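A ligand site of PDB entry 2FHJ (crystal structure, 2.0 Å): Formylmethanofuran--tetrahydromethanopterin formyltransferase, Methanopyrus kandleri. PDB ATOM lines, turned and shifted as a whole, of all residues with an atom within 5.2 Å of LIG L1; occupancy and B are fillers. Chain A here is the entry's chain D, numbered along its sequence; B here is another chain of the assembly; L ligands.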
ATOM      1  N   GLU A  87      16.846 -30.842  22.351  1.00  0.00           N
ATOM      2  CA  GLU A  87      16.529 -29.720  21.485  1.00  0.00           C
ATOM      3  C   GLU A  87      17.600 -28.618  21.556  1.00  0.00           C
ATOM      4  O   GLU A  87      17.864 -27.961  20.564  1.00  0.00           O
ATOM      5  CB  GLU A  87      15.162 -29.135  21.866  1.00  0.00           C
ATOM      6  CG  GLU A  87      14.654 -28.080  20.894  1.00  0.00           C
ATOM      7  CD  GLU A  87      13.997 -28.652  19.635  1.00  0.00           C
ATOM      8  OE1 GLU A  87      14.174 -29.861  19.314  1.00  0.00           O
ATOM      9  OE2 GLU A  87      13.257 -27.869  18.985  1.00  0.00           O
ATOM     10  N   LEU A  90      20.745 -29.855  19.596  1.00  0.00           N
ATOM     11  CA  LEU A  90      20.506 -29.667  18.171  1.00  0.00           C
ATOM     12  C   LEU A  90      20.567 -28.206  17.769  1.00  0.00           C
ATOM     13  O   LEU A  90      21.128 -27.867  16.718  1.00  0.00           O
ATOM     14  CB  LEU A  90      19.137 -30.245  17.818  1.00  0.00           C
ATOM     15  CG  LEU A  90      18.761 -30.297  16.337  1.00  0.00           C
ATOM     16  CD1 LEU A  90      19.477 -31.440  15.630  1.00  0.00           C
ATOM     17  CD2 LEU A  90      17.259 -30.443  16.196  1.00  0.00           C
ATOM     18  N   GLY A  94      23.724 -27.097  15.872  1.00  0.00           N
ATOM     19  CA  GLY A  94      23.230 -26.749  14.536  1.00  0.00           C
ATOM     20  C   GLY A  94      23.375 -25.295  14.129  1.00  0.00           C
ATOM     21  O   GLY A  94      23.697 -25.012  12.978  1.00  0.00           O
ATOM     22  N   GLN A  95      23.106 -24.371  15.051  1.00  0.00           N
ATOM     23  CA  GLN A  95      23.159 -22.933  14.750  1.00  0.00           C
ATOM     24  C   GLN A  95      24.456 -22.270  15.115  1.00  0.00           C
ATOM     25  O   GLN A  95      24.713 -21.163  14.632  1.00  0.00           O
ATOM     26  CB  GLN A  95      22.082 -22.185  15.509  1.00  0.00           C
ATOM     27  CG  GLN A  95      20.665 -22.631  15.177  1.00  0.00           C
ATOM     28  CD  GLN A  95      20.265 -22.192  13.820  1.00  0.00           C
ATOM     29  OE1 GLN A  95      20.010 -21.010  13.577  1.00  0.00           O
ATOM     30  NE2 GLN A  95      20.192 -23.130  12.901  1.00  0.00           N
ATOM     31  N   MET A  98      27.803 -25.696  13.778  1.00  0.00           N
ATOM     32  CA  MET A  98      27.769 -25.980  12.337  1.00  0.00           C
ATOM     33  C   MET A  98      28.169 -24.759  11.504  1.00  0.00           C
ATOM     34  O   MET A  98      28.916 -24.901  10.518  1.00  0.00           O
ATOM     35  CB  MET A  98      26.430 -26.453  11.860  1.00  0.00           C
ATOM     36  CG  MET A  98      26.453 -26.835  10.397  1.00  0.00           C
ATOM     37  SD  MET A  98      25.024 -27.804   9.940  1.00  0.00           S
ATOM     38  CE  MET A  98      23.807 -26.529   9.872  1.00  0.00           C
ATOM     39  N   THR A  99      27.663 -23.582  11.940  1.00  0.00           N
ATOM     40  CA  THR A  99      27.803 -22.335  11.212  1.00  0.00           C
ATOM     41  C   THR A  99      29.184 -21.707  11.423  1.00  0.00           C
ATOM     42  O   THR A  99      29.565 -20.820  10.686  1.00  0.00           O
ATOM     43  CB  THR A  99      26.743 -21.325  11.647  1.00  0.00           C
ATOM     44  OG1 THR A  99      26.870 -21.073  13.035  1.00  0.00           O
ATOM     45  CG2 THR A  99      25.268 -21.842  11.366  1.00  0.00           C
ATOM     46  N   TYR A 122      22.897 -37.255  13.294  1.00  0.00           N
ATOM     47  CA  TYR A 122      21.956 -37.804  12.330  1.00  0.00           C
ATOM     48  C   TYR A 122      20.890 -36.780  12.013  1.00  0.00           C
ATOM     49  O   TYR A 122      20.547 -36.535  10.869  1.00  0.00           O
ATOM     50  CB  TYR A 122      21.327 -39.077  12.873  1.00  0.00           C
ATOM     51  CG  TYR A 122      20.222 -39.637  12.012  1.00  0.00           C
ATOM     52  CD1 TYR A 122      20.511 -40.256  10.805  1.00  0.00           C
ATOM     53  CD2 TYR A 122      18.890 -39.573  12.420  1.00  0.00           C
ATOM     54  CE1 TYR A 122      19.489 -40.791  10.017  1.00  0.00           C
ATOM     55  CE2 TYR A 122      17.869 -40.093  11.642  1.00  0.00           C
ATOM     56  CZ  TYR A 122      18.180 -40.692  10.445  1.00  0.00           C
ATOM     57  OH  TYR A 122      17.151 -41.218   9.686  1.00  0.00           O
ATOM     58  N   LYS A 123      20.376 -36.157  13.057  1.00  0.00           N
ATOM     59  CA  LYS A 123      19.350 -35.135  12.912  1.00  0.00           C
ATOM     60  C   LYS A 123      19.860 -33.874  12.203  1.00  0.00           C
ATOM     61  O   LYS A 123      19.098 -33.234  11.490  1.00  0.00           O
ATOM     62  CB  LYS A 123      18.778 -34.754  14.287  1.00  0.00           C
ATOM     63  CG  LYS A 123      17.878 -35.817  14.895  1.00  0.00           C
ATOM     64  CD  LYS A 123      17.475 -35.483  16.331  1.00  0.00           C
ATOM     65  CE  LYS A 123      16.449 -36.489  16.860  1.00  0.00           C
ATOM     66  NZ  LYS A 123      16.383 -36.458  18.339  1.00  0.00           N
ATOM     67  N   LEU A 124      21.133 -33.536  12.393  1.00  0.00           N
ATOM     68  CA  LEU A 124      21.745 -32.427  11.677  1.00  0.00           C
ATOM     69  C   LEU A 124      22.013 -32.757  10.234  1.00  0.00           C
ATOM     70  O   LEU A 124      21.946 -31.867   9.393  1.00  0.00           O
ATOM     71  CB  LEU A 124      23.052 -31.963  12.343  1.00  0.00           C
ATOM     72  CG  LEU A 124      22.927 -31.230  13.703  1.00  0.00           C
ATOM     73  CD1 LEU A 124      24.299 -30.904  14.280  1.00  0.00           C
ATOM     74  CD2 LEU A 124      22.081 -29.972  13.606  1.00  0.00           C
ATOM     75  N   PHE A 126      20.450 -34.103   7.824  1.00  0.00           N
ATOM     76  CA  PHE A 126      19.393 -33.778   6.850  1.00  0.00           C
ATOM     77  C   PHE A 126      19.519 -32.360   6.244  1.00  0.00           C
ATOM     78  O   PHE A 126      18.925 -32.068   5.205  1.00  0.00           O
ATOM     79  CB  PHE A 126      18.002 -33.954   7.468  1.00  0.00           C
ATOM     80  CG  PHE A 126      17.652 -35.383   7.753  1.00  0.00           C
ATOM     81  CD1 PHE A 126      17.991 -35.980   8.964  1.00  0.00           C
ATOM     82  CD2 PHE A 126      16.998 -36.147   6.805  1.00  0.00           C
ATOM     83  CE1 PHE A 126      17.680 -37.314   9.205  1.00  0.00           C
ATOM     84  CE2 PHE A 126      16.681 -37.459   7.045  1.00  0.00           C
ATOM     85  CZ  PHE A 126      17.022 -38.043   8.245  1.00  0.00           C
ATOM     86  N   PHE A 127      20.275 -31.496   6.911  1.00  0.00           N
ATOM     87  CA  PHE A 127      20.714 -30.216   6.338  1.00  0.00           C
ATOM     88  C   PHE A 127      21.459 -30.382   4.992  1.00  0.00           C
ATOM     89  O   PHE A 127      21.385 -29.485   4.150  1.00  0.00           O
ATOM     90  CB  PHE A 127      21.602 -29.496   7.361  1.00  0.00           C
ATOM     91  CG  PHE A 127      21.935 -28.063   7.005  1.00  0.00           C
ATOM     92  CD1 PHE A 127      23.191 -27.713   6.521  1.00  0.00           C
ATOM     93  CD2 PHE A 127      20.997 -27.055   7.176  1.00  0.00           C
ATOM     94  CE1 PHE A 127      23.513 -26.390   6.200  1.00  0.00           C
ATOM     95  CE2 PHE A 127      21.297 -25.738   6.854  1.00  0.00           C
ATOM     96  CZ  PHE A 127      22.580 -25.404   6.373  1.00  0.00           C
ATOM     97  N   SER B  46      21.008 -16.898  14.414  1.00  0.00           N
ATOM     98  CA  SER B  46      19.955 -16.901  13.417  1.00  0.00           C
ATOM     99  C   SER B  46      18.658 -17.251  14.139  1.00  0.00           C
ATOM    100  O   SER B  46      18.699 -18.050  15.053  1.00  0.00           O
ATOM    101  CB  SER B  46      20.256 -17.968  12.373  1.00  0.00           C
ATOM    102  OG  SER B  46      19.086 -18.422  11.683  1.00  0.00           O
ATOM    103  N   ILE B  48      16.373 -18.950  12.812  1.00  0.00           N
ATOM    104  CA  ILE B  48      16.010 -20.277  12.349  1.00  0.00           C
ATOM    105  C   ILE B  48      15.872 -21.255  13.534  1.00  0.00           C
ATOM    106  O   ILE B  48      14.799 -21.847  13.718  1.00  0.00           O
ATOM    107  CB  ILE B  48      17.015 -20.799  11.285  1.00  0.00           C
ATOM    108  CG1 ILE B  48      16.875 -19.988   9.993  1.00  0.00           C
ATOM    109  CG2 ILE B  48      16.801 -22.272  10.987  1.00  0.00           C
ATOM    110  CD1 ILE B  48      17.919 -20.308   8.921  1.00  0.00           C
ATOM    111  N   MET B  49      16.923 -21.418  14.329  1.00  0.00           N
ATOM    112  CA  MET B  49      16.839 -22.257  15.530  1.00  0.00           C
ATOM    113  C   MET B  49      17.476 -21.662  16.786  1.00  0.00           C
ATOM    114  O   MET B  49      17.627 -22.375  17.773  1.00  0.00           O
ATOM    115  CB  MET B  49      17.475 -23.635  15.282  1.00  0.00           C
ATOM    116  CG  MET B  49      16.741 -24.536  14.296  1.00  0.00           C
ATOM    117  SD  MET B  49      17.187 -26.267  14.527  1.00  0.00           S
ATOM    118  CE  MET B  49      19.012 -26.205  14.499  1.00  0.00           C
ATOM    119  N   TYR B 170      29.051 -13.156  -0.045  1.00  0.00           N
ATOM    120  CA  TYR B 170      29.791 -14.381  -0.025  1.00  0.00           C
ATOM    121  C   TYR B 170      31.222 -14.099  -0.445  1.00  0.00           C
ATOM    122  O   TYR B 170      31.420 -13.319  -1.357  1.00  0.00           O
ATOM    123  CB  TYR B 170      29.232 -15.334  -1.048  1.00  0.00           C
ATOM    124  CG  TYR B 170      27.924 -15.961  -0.654  1.00  0.00           C
ATOM    125  CD1 TYR B 170      26.732 -15.496  -1.170  1.00  0.00           C
ATOM    126  CD2 TYR B 170      27.883 -17.033   0.211  1.00  0.00           C
ATOM    127  CE1 TYR B 170      25.522 -16.099  -0.832  1.00  0.00           C
ATOM    128  CE2 TYR B 170      26.664 -17.642   0.549  1.00  0.00           C
ATOM    129  CZ  TYR B 170      25.503 -17.166   0.023  1.00  0.00           C
ATOM    130  OH  TYR B 170      24.298 -17.775   0.372  1.00  0.00           O
ATOM    131  N   PHE B 200      26.725 -14.192  13.352  1.00  0.00           N
ATOM    132  CA  PHE B 200      27.272 -15.546  13.318  1.00  0.00           C
ATOM    133  C   PHE B 200      28.637 -15.661  14.027  1.00  0.00           C
ATOM    134  O   PHE B 200      29.269 -14.647  14.329  1.00  0.00           O
ATOM    135  CB  PHE B 200      27.320 -16.064  11.863  1.00  0.00           C
ATOM    136  CG  PHE B 200      25.965 -16.426  11.319  1.00  0.00           C
ATOM    137  CD1 PHE B 200      25.158 -15.455  10.747  1.00  0.00           C
ATOM    138  CD2 PHE B 200      25.473 -17.716  11.419  1.00  0.00           C
ATOM    139  CE1 PHE B 200      23.888 -15.764  10.275  1.00  0.00           C
ATOM    140  CE2 PHE B 200      24.210 -18.032  10.948  1.00  0.00           C
ATOM    141  CZ  PHE B 200      23.411 -17.056  10.366  1.00  0.00           C
ATOM    142  N   VAL B 205      29.598 -17.209   8.520  1.00  0.00           N
ATOM    143  CA  VAL B 205      28.738 -18.356   8.283  1.00  0.00           C
ATOM    144  C   VAL B 205      29.544 -19.341   7.462  1.00  0.00           C
ATOM    145  O   VAL B 205      29.851 -19.072   6.301  1.00  0.00           O
ATOM    146  CB  VAL B 205      27.494 -17.966   7.456  1.00  0.00           C
ATOM    147  CG1 VAL B 205      26.458 -19.063   7.528  1.00  0.00           C
ATOM    148  CG2 VAL B 205      26.909 -16.666   7.952  1.00  0.00           C
ATOM    149  N   SER B 207      28.404 -22.270   6.919  1.00  0.00           N
ATOM    150  CA  SER B 207      27.384 -23.149   6.379  1.00  0.00           C
ATOM    151  C   SER B 207      26.110 -22.403   5.954  1.00  0.00           C
ATOM    152  O   SER B 207      25.017 -22.637   6.490  1.00  0.00           O
ATOM    153  CB  SER B 207      27.037 -24.172   7.435  1.00  0.00           C
ATOM    154  OG  SER B 207      26.399 -23.495   8.501  1.00  0.00           O
ATOM    155  N   ALA B 208      26.242 -21.529   4.964  1.00  0.00           N
ATOM    156  CA  ALA B 208      25.101 -20.815   4.407  1.00  0.00           C
ATOM    157  C   ALA B 208      23.957 -21.735   3.993  1.00  0.00           C
ATOM    158  O   ALA B 208      24.180 -22.886   3.592  1.00  0.00           O
ATOM    159  CB  ALA B 208      25.527 -19.960   3.223  1.00  0.00           C
ATOM    160  N   SER B 209      22.746 -21.176   4.092  1.00  0.00           N
ATOM    161  CA  SER B 209      21.505 -21.922   3.885  1.00  0.00           C
ATOM    162  C   SER B 209      20.597 -21.307   2.824  1.00  0.00           C
ATOM    163  O   SER B 209      20.762 -20.153   2.413  1.00  0.00           O
ATOM    164  CB  SER B 209      20.686 -22.007   5.190  1.00  0.00           C
ATOM    165  OG  SER B 209      20.214 -20.732   5.653  1.00  0.00           O
ATOM    166  N   PHE B 218      10.037 -31.142   6.530  1.00  0.00           N
ATOM    167  CA  PHE B 218      10.072 -30.626   7.910  1.00  0.00           C
ATOM    168  C   PHE B 218      11.093 -29.499   8.147  1.00  0.00           C
ATOM    169  O   PHE B 218      11.186 -28.972   9.268  1.00  0.00           O
ATOM    170  CB  PHE B 218      10.322 -31.780   8.903  1.00  0.00           C
ATOM    171  CG  PHE B 218      11.457 -32.694   8.518  1.00  0.00           C
ATOM    172  CD1 PHE B 218      12.771 -32.421   8.913  1.00  0.00           C
ATOM    173  CD2 PHE B 218      11.210 -33.845   7.761  1.00  0.00           C
ATOM    174  CE1 PHE B 218      13.817 -33.261   8.579  1.00  0.00           C
ATOM    175  CE2 PHE B 218      12.249 -34.692   7.406  1.00  0.00           C
ATOM    176  CZ  PHE B 218      13.563 -34.404   7.821  1.00  0.00           C
ATOM    177  N   LEU B 219      11.848 -29.140   7.105  1.00  0.00           N
ATOM    178  CA  LEU B 219      12.953 -28.188   7.235  1.00  0.00           C
ATOM    179  C   LEU B 219      12.552 -26.831   6.694  1.00  0.00           C
ATOM    180  O   LEU B 219      12.060 -26.750   5.572  1.00  0.00           O
ATOM    181  CB  LEU B 219      14.190 -28.708   6.483  1.00  0.00           C
ATOM    182  CG  LEU B 219      14.923 -29.944   7.005  1.00  0.00           C
ATOM    183  CD1 LEU B 219      16.193 -30.164   6.210  1.00  0.00           C
ATOM    184  CD2 LEU B 219      15.270 -29.813   8.470  1.00  0.00           C
ATOM    185  N   ALA B 221      14.935 -24.476   6.549  1.00  0.00           N
ATOM    186  CA  ALA B 221      16.195 -24.098   5.904  1.00  0.00           C
ATOM    187  C   ALA B 221      17.046 -25.328   5.710  1.00  0.00           C
ATOM    188  O   ALA B 221      16.913 -26.306   6.444  1.00  0.00           O
ATOM    189  CB  ALA B 221      16.955 -23.071   6.734  1.00  0.00           C
ATOM    190  N   GLU B 245      29.980 -16.960   3.966  1.00  0.00           N
ATOM    191  CA  GLU B 245      29.046 -15.863   3.932  1.00  0.00           C
ATOM    192  C   GLU B 245      29.267 -14.993   5.153  1.00  0.00           C
ATOM    193  O   GLU B 245      29.464 -15.484   6.251  1.00  0.00           O
ATOM    194  CB  GLU B 245      27.601 -16.356   3.902  1.00  0.00           C
ATOM    195  CG  GLU B 245      26.630 -15.287   3.486  1.00  0.00           C
ATOM    196  CD  GLU B 245      25.214 -15.722   3.545  1.00  0.00           C
ATOM    197  OE1 GLU B 245      24.914 -16.840   4.017  1.00  0.00           O
ATOM    198  OE2 GLU B 245      24.387 -14.915   3.090  1.00  0.00           O
ATOM    199  N   VAL B 247      27.016 -12.370   7.199  1.00  0.00           N
ATOM    200  CA  VAL B 247      25.659 -11.826   7.331  1.00  0.00           C
ATOM    201  C   VAL B 247      25.592 -10.647   8.301  1.00  0.00           C
ATOM    202  O   VAL B 247      26.084 -10.728   9.414  1.00  0.00           O
ATOM    203  CB  VAL B 247      24.676 -12.897   7.765  1.00  0.00           C
ATOM    204  CG1 VAL B 247      23.304 -12.291   7.994  1.00  0.00           C
ATOM    205  CG2 VAL B 247      24.629 -13.957   6.724  1.00  0.00           C
HETATM  206  C1  LIG L   1      23.008 -19.488   7.881  1.00  0.00           C
HETATM  207  O1  LIG L   1      21.887 -20.169  10.063  1.00  0.00           O
HETATM  208  C2  LIG L   1      22.513 -20.490   8.828  1.00  0.00           C
HETATM  209  O2  LIG L   1      20.460 -24.005  10.423  1.00  0.00           O
HETATM  210  C3  LIG L   1      22.597 -21.806   8.638  1.00  0.00           C
HETATM  211  O3  LIG L   1      15.223 -30.400  12.278  1.00  0.00           O
HETATM  212  C4  LIG L   1      22.004 -22.371   9.799  1.00  0.00           C
HETATM  213  O4  LIG L   1      12.760 -35.242  15.632  1.00  0.00           O
HETATM  214  C5  LIG L   1      21.599 -21.348  10.619  1.00  0.00           C
HETATM  215  O5  LIG L   1      14.122 -33.592  16.091  1.00  0.00           O
HETATM  216  C6  LIG L   1      19.169 -27.982  10.456  1.00  0.00           C
HETATM  217  N1  LIG L   1      13.600 -35.367  12.885  1.00  0.00           N
HETATM  218  C7  LIG L   1      14.378 -36.353  12.434  1.00  0.00           C
HETATM  219  O6  LIG L   1      15.104 -36.131  11.458  1.00  0.00           O
HETATM  220  C8  LIG L   1      14.721 -37.584  13.306  1.00  0.00           C
HETATM  221  C9  LIG L   1      14.177 -34.295  13.743  1.00  0.00           C
HETATM  222  C10 LIG L   1      13.679 -34.342  15.214  1.00  0.00           C
HETATM  223  C11 LIG L   1      15.997 -31.339  12.085  1.00  0.00           C
HETATM  224  C12 LIG L   1      15.510 -32.806  12.223  1.00  0.00           C
HETATM  225  C13 LIG L   1      14.212 -32.909  13.063  1.00  0.00           C
HETATM  226  N2  LIG L   1      17.159 -31.078  11.500  1.00  0.00           N
HETATM  227  C14 LIG L   1      17.808 -29.759  11.688  1.00  0.00           C
HETATM  228  C15 LIG L   1      18.695 -29.462  10.466  1.00  0.00           C
HETATM  229  C16 LIG L   1      18.357 -26.959   9.921  1.00  0.00           C
HETATM  230  C17 LIG L   1      18.797 -25.625   9.917  1.00  0.00           C
HETATM  231  C18 LIG L   1      20.423 -27.655  10.986  1.00  0.00           C
HETATM  232  C19 LIG L   1      20.865 -26.307  10.971  1.00  0.00           C
HETATM  233  C20 LIG L   1      20.067 -25.287  10.427  1.00  0.00           C
HETATM  234  C21 LIG L   1      21.849 -23.767  10.062  1.00  0.00           C
HETATM  235  N3  LIG L   1      22.010 -19.106   6.847  1.00  0.00           N
HETATM  236  C22 LIG L   1      22.346 -18.103   5.942  1.00  0.00           C
HETATM  237  O7  LIG L   1      22.685 -18.334   4.768  1.00  0.00           O
HETATM  238  N1  LG2 L   2      16.053 -15.551   5.876  1.00  0.00           N
HETATM  239  C1  LG2 L   2      15.956 -16.977   5.582  1.00  0.00           C
HETATM  240  C2  LG2 L   2      15.552 -17.904   6.781  1.00  0.00           C
HETATM  241  C3  LG2 L   2      17.279 -17.461   4.994  1.00  0.00           C
HETATM  242  N2  LG2 L   2      18.550 -17.002   5.648  1.00  0.00           N
HETATM  243  C4  LG2 L   2      19.561 -16.713   4.634  1.00  0.00           C
HETATM  244  C5  LG2 L   2      19.606 -17.417   3.468  1.00  0.00           C
HETATM  245  N3  LG2 L   2      20.627 -17.048   2.500  1.00  0.00           N
HETATM  246  C6  LG2 L   2      21.517 -16.044   2.757  1.00  0.00           C
HETATM  247  N4  LG2 L   2      22.436 -15.742   1.867  1.00  0.00           N
HETATM  248  N5  LG2 L   2      21.486 -15.357   3.903  1.00  0.00           N
HETATM  249  C7  LG2 L   2      20.581 -15.615   4.852  1.00  0.00           C
HETATM  250  O1  LG2 L   2      20.596 -14.965   5.883  1.00  0.00           O
HETATM  251  N6  LG2 L   2      18.641 -18.502   3.172  1.00  0.00           N
HETATM  252  C8  LG2 L   2      17.757 -18.725   4.300  1.00  0.00           C
HETATM  253  C9  LG2 L   2      17.511 -20.185   4.712  1.00  0.00           C
HETATM  254  C10 LG2 L   2      18.383 -17.177   7.112  1.00  0.00           C
HETATM  255  O2  LG2 L   2      18.097 -16.231   7.862  1.00  0.00           O
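NE2 of Gln 95 is in hydrogen-bond range of O2 of LIG L1, at 2.6 Å.
An oxygen (O7) of LIG L1 sits at hydrogen-bond distance from the backbone NH (N) of Ser 209 of chain B (2.9 Å).
N3 of LIG L1 is in hydrogen-bond range of OG of Ser 209 of chain B (2.7 Å).
The backbone carbonyl oxygen of Lys 123 lies within hydrogen-bond range of a nitrogen (N2) of LIG L1 (2.9 Å).
The backbone carbonyl oxygen of Ser 209 of chain B lies within hydrogen-bond range of a nitrogen (N6) of LG2 L2 (2.8 Å).
OE2 of Glu 245 of chain B lies within hydrogen-bond range of N4 of LG2 L2 (2.4 Å).
A nitrogen (N4) of LG2 L2 lies within hydrogen-bond range of the side-chain hydroxyl (OH) of Tyr 170 of chain B.
An oxygen (O7) of LIG L1 lies close to a nitrogen (N5) of LG2 L2 (3.3 Å).
OE1 of Gln 95 lies close to OG of Ser 46 of chain B.
The backbone carbonyl oxygen (O) of Gln 95 lies within hydrogen-bond range of the side-chain hydroxyl (OG1) of Thr 99, at 2.7 Å.
The backbone NH (N) of Met 49 of chain B sits at hydrogen-bond distance from the side-chain amide oxygen (OE1) of Gln 95.
The backbone NH (N) of Val 205 of chain B is in hydrogen-bond range of the backbone carbonyl oxygen (O) of Glu 245 of chain B (2.9 Å).
The backbone NH (N) of Ile 48 of chain B is in hydrogen-bond range of the side-chain hydroxyl (OG) of Ser 46 of chain B (3.0 Å).
O7 of LIG L1 lies close to OE1 of Glu 245 of chain B, at 2.8 Å.
Residues that only touch LIG L1: Gly 94, Met 98, Thr 99, Leu 124, Phe 126, Phe 127, Ser 46 of chain B, Met 49 of chain B, Phe 200 of chain B, Val 205 of chain B, Ser 207 of chain B, Ala 208 of chain B, Leu 219 of chain B and Ala 221 of chain B.
Hydrophobic or aromatic side chains that line LIG L1: Met 98, Leu 124, Phe 126, Phe 127, Met 49 of chain B, Phe 200 of chain B, Val 205 of chain B, Ala 208 of chain B and Leu 219 of chain B.
The nearest printed residue that does not touch LIG L1 is Phe 218 of chain B (4.04 Å).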
